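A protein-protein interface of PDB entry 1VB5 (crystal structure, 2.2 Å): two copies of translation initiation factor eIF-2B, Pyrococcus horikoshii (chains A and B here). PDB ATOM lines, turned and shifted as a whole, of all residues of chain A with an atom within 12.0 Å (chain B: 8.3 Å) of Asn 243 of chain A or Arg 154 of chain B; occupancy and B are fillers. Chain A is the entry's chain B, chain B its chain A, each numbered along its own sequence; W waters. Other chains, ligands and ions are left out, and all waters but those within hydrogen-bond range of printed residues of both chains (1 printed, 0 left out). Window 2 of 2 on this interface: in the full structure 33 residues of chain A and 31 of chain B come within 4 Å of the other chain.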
ATOM      1  N   ASP A 238       1.678 -20.506  -7.551  1.00  0.00           N
ATOM      2  CA  ASP A 238       0.483 -19.963  -6.912  1.00  0.00           C
ATOM      3  C   ASP A 238      -0.578 -19.667  -7.968  1.00  0.00           C
ATOM      4  O   ASP A 238      -0.258 -19.241  -9.080  1.00  0.00           O
ATOM      5  CB  ASP A 238       0.828 -18.682  -6.153  1.00  0.00           C
ATOM      6  CG  ASP A 238       1.496 -18.955  -4.823  1.00  0.00           C
ATOM      7  OD1 ASP A 238       2.257 -19.942  -4.732  1.00  0.00           O
ATOM      8  OD2 ASP A 238       1.269 -18.180  -3.868  1.00  0.00           O
ATOM      9  N   LEU A 239      -1.839 -19.899  -7.618  1.00  0.00           N
ATOM     10  CA  LEU A 239      -2.943 -19.652  -8.543  1.00  0.00           C
ATOM     11  C   LEU A 239      -4.189 -19.166  -7.808  1.00  0.00           C
ATOM     12  O   LEU A 239      -4.523 -19.659  -6.727  1.00  0.00           O
ATOM     13  CB  LEU A 239      -3.269 -20.928  -9.328  1.00  0.00           C
ATOM     14  CG  LEU A 239      -4.509 -20.913 -10.233  1.00  0.00           C
ATOM     15  CD1 LEU A 239      -4.319 -19.928 -11.377  1.00  0.00           C
ATOM     16  CD2 LEU A 239      -4.753 -22.308 -10.775  1.00  0.00           C
ATOM     17  N   ILE A 240      -4.866 -18.189  -8.403  1.00  0.00           N
ATOM     18  CA  ILE A 240      -6.087 -17.623  -7.839  1.00  0.00           C
ATOM     19  C   ILE A 240      -7.065 -17.260  -8.954  1.00  0.00           C
ATOM     20  O   ILE A 240      -6.699 -16.602  -9.926  1.00  0.00           O
ATOM     21  CB  ILE A 240      -5.800 -16.349  -7.010  1.00  0.00           C
ATOM     22  CG1 ILE A 240      -4.919 -16.689  -5.810  1.00  0.00           C
ATOM     23  CG2 ILE A 240      -7.108 -15.738  -6.520  1.00  0.00           C
ATOM     24  CD1 ILE A 240      -4.632 -15.501  -4.905  1.00  0.00           C
ATOM     25  N   ARG A 241      -8.306 -17.711  -8.809  1.00  0.00           N
ATOM     26  CA  ARG A 241      -9.362 -17.430  -9.778  1.00  0.00           C
ATOM     27  C   ARG A 241     -10.574 -17.043  -8.945  1.00  0.00           C
ATOM     28  O   ARG A 241     -10.976 -17.780  -8.044  1.00  0.00           O
ATOM     29  CB  ARG A 241      -9.659 -18.666 -10.626  1.00  0.00           C
ATOM     30  CG  ARG A 241     -10.776 -18.468 -11.645  1.00  0.00           C
ATOM     31  CD  ARG A 241     -10.915 -19.684 -12.549  1.00  0.00           C
ATOM     32  NE  ARG A 241      -9.791 -19.818 -13.474  1.00  0.00           N
ATOM     33  CZ  ARG A 241      -9.574 -19.009 -14.509  1.00  0.00           C
ATOM     34  NH1 ARG A 241     -10.406 -18.004 -14.758  1.00  0.00           N
ATOM     35  NH2 ARG A 241      -8.530 -19.206 -15.301  1.00  0.00           N
ATOM     36  N   GLY A 242     -11.160 -15.889  -9.247  1.00  0.00           N
ATOM     37  CA  GLY A 242     -12.276 -15.421  -8.452  1.00  0.00           C
ATOM     38  C   GLY A 242     -11.598 -14.960  -7.174  1.00  0.00           C
ATOM     39  O   GLY A 242     -10.586 -14.264  -7.227  1.00  0.00           O
ATOM     40  N   ASN A 243     -12.126 -15.345  -6.024  1.00  0.00           N
ATOM     41  CA  ASN A 243     -11.498 -14.961  -4.764  1.00  0.00           C
ATOM     42  C   ASN A 243     -10.991 -16.248  -4.122  1.00  0.00           C
ATOM     43  O   ASN A 243     -10.703 -16.296  -2.925  1.00  0.00           O
ATOM     44  CB  ASN A 243     -12.521 -14.272  -3.849  1.00  0.00           C
ATOM     45  CG  ASN A 243     -13.710 -15.177  -3.493  1.00  0.00           C
ATOM     46  OD1 ASN A 243     -13.571 -16.136  -2.729  1.00  0.00           O
ATOM     47  ND2 ASN A 243     -14.882 -14.872  -4.054  1.00  0.00           N
ATOM     48  N   VAL A 244     -10.864 -17.285  -4.945  1.00  0.00           N
ATOM     49  CA  VAL A 244     -10.458 -18.605  -4.480  1.00  0.00           C
ATOM     50  C   VAL A 244      -9.033 -19.035  -4.810  1.00  0.00           C
ATOM     51  O   VAL A 244      -8.584 -18.935  -5.953  1.00  0.00           O
ATOM     52  CB  VAL A 244     -11.426 -19.672  -5.040  1.00  0.00           C
ATOM     53  CG1 VAL A 244     -11.172 -21.014  -4.378  1.00  0.00           C
ATOM     54  CG2 VAL A 244     -12.865 -19.221  -4.831  1.00  0.00           C
ATOM     55  N   ARG A 245      -8.325 -19.517  -3.793  1.00  0.00           N
ATOM     56  CA  ARG A 245      -6.966 -20.000  -3.979  1.00  0.00           C
ATOM     57  C   ARG A 245      -7.074 -21.406  -4.555  1.00  0.00           C
ATOM     58  O   ARG A 245      -7.856 -22.231  -4.076  1.00  0.00           O
ATOM     59  CB  ARG A 245      -6.210 -20.015  -2.649  1.00  0.00           C
ATOM     60  CG  ARG A 245      -5.794 -18.628  -2.187  1.00  0.00           C
ATOM     61  CD  ARG A 245      -4.927 -18.667  -0.937  1.00  0.00           C
ATOM     62  NE  ARG A 245      -4.115 -17.455  -0.811  1.00  0.00           N
ATOM     63  CZ  ARG A 245      -4.606 -16.219  -0.746  1.00  0.00           C
ATOM     64  NH1 ARG A 245      -5.917 -16.012  -0.790  1.00  0.00           N
ATOM     65  NH2 ARG A 245      -3.783 -15.184  -0.643  1.00  0.00           N
ATOM     66  N   ILE A 246      -6.291 -21.677  -5.589  1.00  0.00           N
ATOM     67  CA  ILE A 246      -6.344 -22.974  -6.236  1.00  0.00           C
ATOM     68  C   ILE A 246      -5.002 -23.693  -6.213  1.00  0.00           C
ATOM     69  O   ILE A 246      -3.982 -23.139  -6.616  1.00  0.00           O
ATOM     70  CB  ILE A 246      -6.831 -22.803  -7.694  1.00  0.00           C
ATOM     71  CG1 ILE A 246      -8.202 -22.110  -7.687  1.00  0.00           C
ATOM     72  CG2 ILE A 246      -6.902 -24.160  -8.402  1.00  0.00           C
ATOM     73  CD1 ILE A 246      -8.668 -21.629  -9.050  1.00  0.00           C
ATOM     74  N   ARG A 247      -5.006 -24.922  -5.714  1.00  0.00           N
ATOM     75  CA  ARG A 247      -3.789 -25.723  -5.675  1.00  0.00           C
ATOM     76  C   ARG A 247      -3.388 -25.876  -7.148  1.00  0.00           C
ATOM     77  O   ARG A 247      -4.244 -26.119  -8.005  1.00  0.00           O
ATOM     78  CB  ARG A 247      -4.083 -27.090  -5.049  1.00  0.00           C
ATOM     79  CG  ARG A 247      -2.864 -27.956  -4.801  1.00  0.00           C
ATOM     80  CD  ARG A 247      -1.941 -27.358  -3.738  1.00  0.00           C
ATOM     81  NE  ARG A 247      -0.726 -28.156  -3.589  1.00  0.00           N
ATOM     82  CZ  ARG A 247      -0.651 -29.294  -2.905  1.00  0.00           C
ATOM     83  NH1 ARG A 247      -1.725 -29.778  -2.291  1.00  0.00           N
ATOM     84  NH2 ARG A 247       0.496 -29.958  -2.846  1.00  0.00           N
ATOM     85  N   ILE B  18     -23.925 -22.279 -13.759  1.00  0.00           N
ATOM     86  CA  ILE B  18     -23.516 -22.826 -12.466  1.00  0.00           C
ATOM     87  C   ILE B  18     -24.466 -23.862 -11.870  1.00  0.00           C
ATOM     88  O   ILE B  18     -24.160 -25.057 -11.848  1.00  0.00           O
ATOM     89  CB  ILE B  18     -23.319 -21.699 -11.424  1.00  0.00           C
ATOM     90  CG1 ILE B  18     -22.042 -20.917 -11.733  1.00  0.00           C
ATOM     91  CG2 ILE B  18     -23.253 -22.285 -10.019  1.00  0.00           C
ATOM     92  CD1 ILE B  18     -22.093 -20.139 -13.019  1.00  0.00           C
ATOM     93  N   PHE B 118     -20.383 -28.986  -9.746  1.00  0.00           N
ATOM     94  CA  PHE B 118     -21.255 -28.555  -8.658  1.00  0.00           C
ATOM     95  C   PHE B 118     -22.571 -29.312  -8.619  1.00  0.00           C
ATOM     96  O   PHE B 118     -23.325 -29.313  -9.590  1.00  0.00           O
ATOM     97  CB  PHE B 118     -21.579 -27.062  -8.754  1.00  0.00           C
ATOM     98  CG  PHE B 118     -22.647 -26.622  -7.785  1.00  0.00           C
ATOM     99  CD1 PHE B 118     -22.400 -26.616  -6.413  1.00  0.00           C
ATOM    100  CD2 PHE B 118     -23.924 -26.289  -8.237  1.00  0.00           C
ATOM    101  CE1 PHE B 118     -23.413 -26.291  -5.506  1.00  0.00           C
ATOM    102  CE2 PHE B 118     -24.944 -25.962  -7.338  1.00  0.00           C
ATOM    103  CZ  PHE B 118     -24.689 -25.965  -5.970  1.00  0.00           C
ATOM    104  N   LEU B 123     -23.596 -31.169  -2.177  1.00  0.00           N
ATOM    105  CA  LEU B 123     -23.370 -30.123  -1.179  1.00  0.00           C
ATOM    106  C   LEU B 123     -24.200 -30.393   0.079  1.00  0.00           C
ATOM    107  O   LEU B 123     -23.720 -30.202   1.197  1.00  0.00           O
ATOM    108  CB  LEU B 123     -23.731 -28.743  -1.738  1.00  0.00           C
ATOM    109  CG  LEU B 123     -23.708 -27.569  -0.746  1.00  0.00           C
ATOM    110  CD1 LEU B 123     -22.334 -27.439  -0.104  1.00  0.00           C
ATOM    111  CD2 LEU B 123     -24.083 -26.276  -1.471  1.00  0.00           C
ATOM    112  N   ARG B 127     -23.013 -30.957   3.897  1.00  0.00           N
ATOM    113  CA  ARG B 127     -23.492 -30.086   4.962  1.00  0.00           C
ATOM    114  C   ARG B 127     -24.188 -30.874   6.056  1.00  0.00           C
ATOM    115  O   ARG B 127     -24.123 -30.505   7.235  1.00  0.00           O
ATOM    116  CB  ARG B 127     -24.445 -29.034   4.405  1.00  0.00           C
ATOM    117  CG  ARG B 127     -23.736 -27.874   3.768  1.00  0.00           C
ATOM    118  CD  ARG B 127     -24.708 -26.882   3.159  1.00  0.00           C
ATOM    119  NE  ARG B 127     -24.018 -25.640   2.831  1.00  0.00           N
ATOM    120  CZ  ARG B 127     -24.501 -24.697   2.027  1.00  0.00           C
ATOM    121  NH1 ARG B 127     -25.688 -24.847   1.456  1.00  0.00           N
ATOM    122  NH2 ARG B 127     -23.789 -23.604   1.798  1.00  0.00           N
ATOM    123  N   LEU B 140     -12.024 -30.416  -4.319  1.00  0.00           N
ATOM    124  CA  LEU B 140     -12.924 -30.174  -5.437  1.00  0.00           C
ATOM    125  C   LEU B 140     -12.190 -29.505  -6.594  1.00  0.00           C
ATOM    126  O   LEU B 140     -11.141 -28.891  -6.403  1.00  0.00           O
ATOM    127  CB  LEU B 140     -14.079 -29.280  -4.979  1.00  0.00           C
ATOM    128  CG  LEU B 140     -13.633 -27.914  -4.439  1.00  0.00           C
ATOM    129  CD1 LEU B 140     -14.157 -26.810  -5.347  1.00  0.00           C
ATOM    130  CD2 LEU B 140     -14.140 -27.725  -3.016  1.00  0.00           C
ATOM    131  N   ASP B 146     -16.957 -23.037 -17.124  1.00  0.00           N
ATOM    132  CA  ASP B 146     -17.754 -22.068 -16.363  1.00  0.00           C
ATOM    133  C   ASP B 146     -17.395 -21.960 -14.886  1.00  0.00           C
ATOM    134  O   ASP B 146     -17.866 -21.062 -14.183  1.00  0.00           O
ATOM    135  CB  ASP B 146     -19.236 -22.397 -16.522  1.00  0.00           C
ATOM    136  CG  ASP B 146     -19.660 -22.418 -17.977  1.00  0.00           C
ATOM    137  OD1 ASP B 146     -19.529 -21.374 -18.642  1.00  0.00           O
ATOM    138  OD2 ASP B 146     -20.112 -23.477 -18.457  1.00  0.00           O
ATOM    139  N   TYR B 147     -16.566 -22.884 -14.418  1.00  0.00           N
ATOM    140  CA  TYR B 147     -16.103 -22.876 -13.038  1.00  0.00           C
ATOM    141  C   TYR B 147     -17.179 -23.009 -11.962  1.00  0.00           C
ATOM    142  O   TYR B 147     -17.088 -22.374 -10.910  1.00  0.00           O
ATOM    143  CB  TYR B 147     -15.285 -21.608 -12.808  1.00  0.00           C
ATOM    144  CG  TYR B 147     -14.129 -21.500 -13.775  1.00  0.00           C
ATOM    145  CD1 TYR B 147     -13.952 -20.362 -14.563  1.00  0.00           C
ATOM    146  CD2 TYR B 147     -13.219 -22.548 -13.914  1.00  0.00           C
ATOM    147  CE1 TYR B 147     -12.890 -20.274 -15.473  1.00  0.00           C
ATOM    148  CE2 TYR B 147     -12.155 -22.472 -14.815  1.00  0.00           C
ATOM    149  CZ  TYR B 147     -11.998 -21.335 -15.591  1.00  0.00           C
ATOM    150  OH  TYR B 147     -10.960 -21.268 -16.485  1.00  0.00           O
ATOM    151  N   GLU B 148     -18.182 -23.845 -12.213  1.00  0.00           N
ATOM    152  CA  GLU B 148     -19.243 -24.041 -11.234  1.00  0.00           C
ATOM    153  C   GLU B 148     -18.625 -24.577  -9.940  1.00  0.00           C
ATOM    154  O   GLU B 148     -19.222 -24.484  -8.871  1.00  0.00           O
ATOM    155  CB  GLU B 148     -20.298 -25.023 -11.757  1.00  0.00           C
ATOM    156  CG  GLU B 148     -19.772 -26.422 -12.010  1.00  0.00           C
ATOM    157  CD  GLU B 148     -19.272 -26.625 -13.432  1.00  0.00           C
ATOM    158  OE1 GLU B 148     -18.941 -25.628 -14.115  1.00  0.00           O
ATOM    159  OE2 GLU B 148     -19.205 -27.793 -13.869  1.00  0.00           O
ATOM    160  N   GLY B 149     -17.423 -25.136 -10.049  1.00  0.00           N
ATOM    161  CA  GLY B 149     -16.738 -25.665  -8.882  1.00  0.00           C
ATOM    162  C   GLY B 149     -16.400 -24.580  -7.868  1.00  0.00           C
ATOM    163  O   GLY B 149     -16.396 -24.821  -6.658  1.00  0.00           O
ATOM    164  N   LEU B 150     -16.105 -23.380  -8.356  1.00  0.00           N
ATOM    165  CA  LEU B 150     -15.776 -22.278  -7.464  1.00  0.00           C
ATOM    166  C   LEU B 150     -17.013 -21.874  -6.668  1.00  0.00           C
ATOM    167  O   LEU B 150     -16.900 -21.321  -5.578  1.00  0.00           O
ATOM    168  CB  LEU B 150     -15.239 -21.079  -8.257  1.00  0.00           C
ATOM    169  CG  LEU B 150     -13.939 -21.316  -9.031  1.00  0.00           C
ATOM    170  CD1 LEU B 150     -13.408 -19.974  -9.544  1.00  0.00           C
ATOM    171  CD2 LEU B 150     -12.907 -21.984  -8.126  1.00  0.00           C
ATOM    172  N   HIS B 151     -18.192 -22.149  -7.220  1.00  0.00           N
ATOM    173  CA  HIS B 151     -19.439 -21.842  -6.530  1.00  0.00           C
ATOM    174  C   HIS B 151     -19.528 -22.780  -5.322  1.00  0.00           C
ATOM    175  O   HIS B 151     -19.901 -22.368  -4.219  1.00  0.00           O
ATOM    176  CB  HIS B 151     -20.638 -22.068  -7.457  1.00  0.00           C
ATOM    177  CG  HIS B 151     -21.960 -22.019  -6.751  1.00  0.00           C
ATOM    178  ND1 HIS B 151     -22.373 -20.926  -6.019  1.00  0.00           N
ATOM    179  CD2 HIS B 151     -22.950 -22.936  -6.651  1.00  0.00           C
ATOM    180  CE1 HIS B 151     -23.562 -21.173  -5.499  1.00  0.00           C
ATOM    181  NE2 HIS B 151     -23.934 -22.385  -5.866  1.00  0.00           N
ATOM    182  N   LEU B 152     -19.185 -24.045  -5.541  1.00  0.00           N
ATOM    183  CA  LEU B 152     -19.189 -25.027  -4.464  1.00  0.00           C
ATOM    184  C   LEU B 152     -18.225 -24.556  -3.383  1.00  0.00           C
ATOM    185  O   LEU B 152     -18.543 -24.598  -2.195  1.00  0.00           O
ATOM    186  CB  LEU B 152     -18.737 -26.400  -4.970  1.00  0.00           C
ATOM    187  CG  LEU B 152     -18.534 -27.457  -3.878  1.00  0.00           C
ATOM    188  CD1 LEU B 152     -19.840 -27.649  -3.117  1.00  0.00           C
ATOM    189  CD2 LEU B 152     -18.076 -28.777  -4.499  1.00  0.00           C
ATOM    190  N   ALA B 153     -17.047 -24.103  -3.801  1.00  0.00           N
ATOM    191  CA  ALA B 153     -16.045 -23.632  -2.854  1.00  0.00           C
ATOM    192  C   ALA B 153     -16.573 -22.510  -1.960  1.00  0.00           C
ATOM    193  O   ALA B 153     -16.329 -22.501  -0.755  1.00  0.00           O
ATOM    194  CB  ALA B 153     -14.801 -23.166  -3.596  1.00  0.00           C
ATOM    195  N   ARG B 154     -17.298 -21.564  -2.548  1.00  0.00           N
ATOM    196  CA  ARG B 154     -17.835 -20.449  -1.777  1.00  0.00           C
ATOM    197  C   ARG B 154     -18.922 -20.910  -0.810  1.00  0.00           C
ATOM    198  O   ARG B 154     -19.095 -20.325   0.261  1.00  0.00           O
ATOM    199  CB  ARG B 154     -18.364 -19.370  -2.724  1.00  0.00           C
ATOM    200  CG  ARG B 154     -17.259 -18.789  -3.593  1.00  0.00           C
ATOM    201  CD  ARG B 154     -17.773 -17.824  -4.643  1.00  0.00           C
ATOM    202  NE  ARG B 154     -16.680 -17.429  -5.528  1.00  0.00           N
ATOM    203  CZ  ARG B 154     -16.633 -17.696  -6.830  1.00  0.00           C
ATOM    204  NH1 ARG B 154     -17.626 -18.357  -7.415  1.00  0.00           N
ATOM    205  NH2 ARG B 154     -15.584 -17.314  -7.543  1.00  0.00           N
ATOM    206  N   GLU B 155     -19.643 -21.963  -1.182  1.00  0.00           N
ATOM    207  CA  GLU B 155     -20.687 -22.512  -0.322  1.00  0.00           C
ATOM    208  C   GLU B 155     -20.052 -23.255   0.854  1.00  0.00           C
ATOM    209  O   GLU B 155     -20.507 -23.143   1.992  1.00  0.00           O
ATOM    210  CB  GLU B 155     -21.582 -23.478  -1.105  1.00  0.00           C
ATOM    211  CG  GLU B 155     -22.489 -22.816  -2.126  1.00  0.00           C
ATOM    212  CD  GLU B 155     -23.435 -21.806  -1.497  1.00  0.00           C
ATOM    213  OE1 GLU B 155     -24.018 -22.122  -0.433  1.00  0.00           O
ATOM    214  OE2 GLU B 155     -23.601 -20.703  -2.067  1.00  0.00           O
ATOM    215  N   LEU B 156     -19.002 -24.019   0.578  1.00  0.00           N
ATOM    216  CA  LEU B 156     -18.326 -24.766   1.631  1.00  0.00           C
ATOM    217  C   LEU B 156     -17.662 -23.790   2.593  1.00  0.00           C
ATOM    218  O   LEU B 156     -17.629 -24.012   3.803  1.00  0.00           O
ATOM    219  CB  LEU B 156     -17.287 -25.710   1.026  1.00  0.00           C
ATOM    220  CG  LEU B 156     -17.864 -26.851   0.173  1.00  0.00           C
ATOM    221  CD1 LEU B 156     -16.735 -27.679  -0.416  1.00  0.00           C
ATOM    222  CD2 LEU B 156     -18.774 -27.727   1.034  1.00  0.00           C
ATOM    223  N   GLU B 157     -17.144 -22.703   2.037  1.00  0.00           N
ATOM    224  CA  GLU B 157     -16.489 -21.669   2.819  1.00  0.00           C
ATOM    225  C   GLU B 157     -17.519 -21.035   3.758  1.00  0.00           C
ATOM    226  O   GLU B 157     -17.254 -20.826   4.939  1.00  0.00           O
ATOM    227  CB  GLU B 157     -15.910 -20.616   1.878  1.00  0.00           C
ATOM    228  CG  GLU B 157     -14.824 -19.752   2.471  1.00  0.00           C
ATOM    229  CD  GLU B 157     -14.186 -18.866   1.418  1.00  0.00           C
ATOM    230  OE1 GLU B 157     -14.886 -17.971   0.889  1.00  0.00           O
ATOM    231  OE2 GLU B 157     -12.992 -19.073   1.107  1.00  0.00           O
ATOM    232  N   PHE B 158     -18.699 -20.739   3.223  1.00  0.00           N
ATOM    233  CA  PHE B 158     -19.773 -20.148   4.016  1.00  0.00           C
ATOM    234  C   PHE B 158     -20.143 -21.065   5.180  1.00  0.00           C
ATOM    235  O   PHE B 158     -20.445 -20.599   6.280  1.00  0.00           O
ATOM    236  CB  PHE B 158     -21.010 -19.922   3.146  1.00  0.00           C
ATOM    237  CG  PHE B 158     -22.209 -19.438   3.912  1.00  0.00           C
ATOM    238  CD1 PHE B 158     -22.281 -18.122   4.360  1.00  0.00           C
ATOM    239  CD2 PHE B 158     -23.261 -20.303   4.200  1.00  0.00           C
ATOM    240  CE1 PHE B 158     -23.388 -17.671   5.088  1.00  0.00           C
ATOM    241  CE2 PHE B 158     -24.372 -19.867   4.926  1.00  0.00           C
ATOM    242  CZ  PHE B 158     -24.435 -18.546   5.371  1.00  0.00           C
ATOM    243  N   SER B 159     -20.112 -22.371   4.926  1.00  0.00           N
ATOM    244  CA  SER B 159     -20.453 -23.370   5.935  1.00  0.00           C
ATOM    245  C   SER B 159     -19.298 -23.730   6.867  1.00  0.00           C
ATOM    246  O   SER B 159     -19.454 -24.563   7.752  1.00  0.00           O
ATOM    247  CB  SER B 159     -20.965 -24.637   5.252  1.00  0.00           C
ATOM    248  OG  SER B 159     -22.120 -24.361   4.482  1.00  0.00           O
ATOM    249  N   GLY B 160     -18.139 -23.110   6.661  1.00  0.00           N
ATOM    250  CA  GLY B 160     -16.991 -23.388   7.508  1.00  0.00           C
ATOM    251  C   GLY B 160     -16.423 -24.787   7.353  1.00  0.00           C
ATOM    252  O   GLY B 160     -15.957 -25.396   8.320  1.00  0.00           O
ATOM    253  N   ILE B 161     -16.456 -25.301   6.130  1.00  0.00           N
ATOM    254  CA  ILE B 161     -15.942 -26.634   5.846  1.00  0.00           C
ATOM    255  C   ILE B 161     -14.557 -26.528   5.210  1.00  0.00           C
ATOM    256  O   ILE B 161     -14.339 -25.700   4.331  1.00  0.00           O
ATOM    257  CB  ILE B 161     -16.908 -27.385   4.900  1.00  0.00           C
ATOM    258  CG1 ILE B 161     -18.248 -27.593   5.617  1.00  0.00           C
ATOM    259  CG2 ILE B 161     -16.298 -28.714   4.461  1.00  0.00           C
ATOM    260  CD1 ILE B 161     -19.324 -28.251   4.773  1.00  0.00           C
ATOM    261  N   PHE B 163     -11.655 -27.191   2.799  1.00  0.00           N
ATOM    262  CA  PHE B 163     -11.583 -27.649   1.423  1.00  0.00           C
ATOM    263  C   PHE B 163     -10.332 -27.162   0.701  1.00  0.00           C
ATOM    264  O   PHE B 163      -9.661 -26.221   1.133  1.00  0.00           O
ATOM    265  CB  PHE B 163     -12.821 -27.181   0.658  1.00  0.00           C
ATOM    266  CG  PHE B 163     -12.873 -25.695   0.441  1.00  0.00           C
ATOM    267  CD1 PHE B 163     -12.211 -25.110  -0.637  1.00  0.00           C
ATOM    268  CD2 PHE B 163     -13.559 -24.872   1.331  1.00  0.00           C
ATOM    269  CE1 PHE B 163     -12.232 -23.727  -0.826  1.00  0.00           C
ATOM    270  CE2 PHE B 163     -13.587 -23.481   1.154  1.00  0.00           C
ATOM    271  CZ  PHE B 163     -12.922 -22.911   0.075  1.00  0.00           C
ATOM    272  N   VAL B 165      -9.116 -26.531  -3.492  1.00  0.00           N
ATOM    273  CA  VAL B 165      -9.548 -26.493  -4.885  1.00  0.00           C
ATOM    274  C   VAL B 165      -8.380 -26.843  -5.808  1.00  0.00           C
ATOM    275  O   VAL B 165      -7.240 -26.463  -5.544  1.00  0.00           O
ATOM    276  CB  VAL B 165     -10.083 -25.091  -5.272  1.00  0.00           C
ATOM    277  CG1 VAL B 165     -10.679 -25.126  -6.668  1.00  0.00           C
ATOM    278  CG2 VAL B 165     -11.128 -24.631  -4.262  1.00  0.00           C
HETATM  279  O   HOH W   1      -7.441 -24.426  -2.560  1.00  0.00           O
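The side-chain hydroxyl (OH) of Tyr 147 of chain B lies close to the guanidinium group (NH2) of Arg 241 of chain A (3.4 Å). The side-chain amide nitrogen (ND2) of Asn 243 of chain A lies close to the guanidinium group (NE) of Arg 154 of chain B (3.5 Å). The backbone carbonyl oxygen (O) of Val 165 of chain B sits at hydrogen-bond distance from the backbone NH (N) of Arg 247 of chain A (2.7 Å).
The backbone carbonyl oxygen (O) of Leu 239 of chain A sits at hydrogen-bond distance from the backbone NH (N) of Ile 246 of chain A (2.9 Å).
Arg 241 of chain A touches Leu 150 of chain B. CA of Gly 242 of chain A touches NH2 of Arg 154 of chain B, 3.9 Å away. Val 244 of chain A touches Val 165 of chain B. Arg 245 of chain A touches Val 165 of chain B. Val 165 of chain B touches Ile 246 of chain A (O to C, 3.6 Å).
Asn 243 of chain A touches just one residue of chain B: Arg 154. Of chain A, only Gly 242 and Asn 243 come within 4 Å of Arg 154 of chain B. Gly 242 of chain A touches just one residue of chain B: Arg 154. No residue of chain A comes within 4 Å of Gly 149 of chain B. Leu 150 of chain B touches just one residue of chain A: Arg 241 (3.6 Å). No residue of chain A comes within 4 Å of His 151 of chain B. No residue of chain A comes within 4 Å of Leu 152 of chain B. No residue of chain A comes within 4 Å of Glu 155 of chain B. No residue of chain A comes within 4 Å of Phe 158 of chain B. Printed residues of chain A within 4 Å of Tyr 147 of chain B: Arg 241 (3.3 Å). Of the printed residues of chain B, Arg 241 of chain A touches Tyr 147 and Leu 150. Of the printed residues of chain B, Arg 245 of chain A touches Val 165. Leu 239 of chain A touches none of the printed residues of chain B.
Printed residues of chain B that touch a printed residue of chain A: Tyr 147, Leu 150, Arg 154 and Val 165. Hydrophobic or aromatic side chains of chain B that line the printed part of chain A: Tyr 147, Leu 150 and Val 165. Of the 10 printed residues of chain A, 7 touch a printed residue of chain B. Printed residues of chain A that touch a printed residue of chain B: Arg 241, Gly 242, Asn 243, Val 244, Arg 245, Ile 246 and Arg 247. Hydrophobic or aromatic side chains of chain A that line the printed part of chain B: Val 244 and Ile 246. Along chain A the printed residues that touch a printed residue of chain B span positions 241 to 247. Among the printed residues, no Asp or Glu carboxylate lies within 4 Å of a Lys or Arg side-chain nitrogen of the other chain.
No position is printed for both chains. Of the 8 pairs that touch across the chains among the printed residues, none has its exchanged pair printed and touching as well.
Water W1 bridges O of Arg 245 of chain A (2.7 Å) and N of Val 165 of chain B (2.8 Å).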
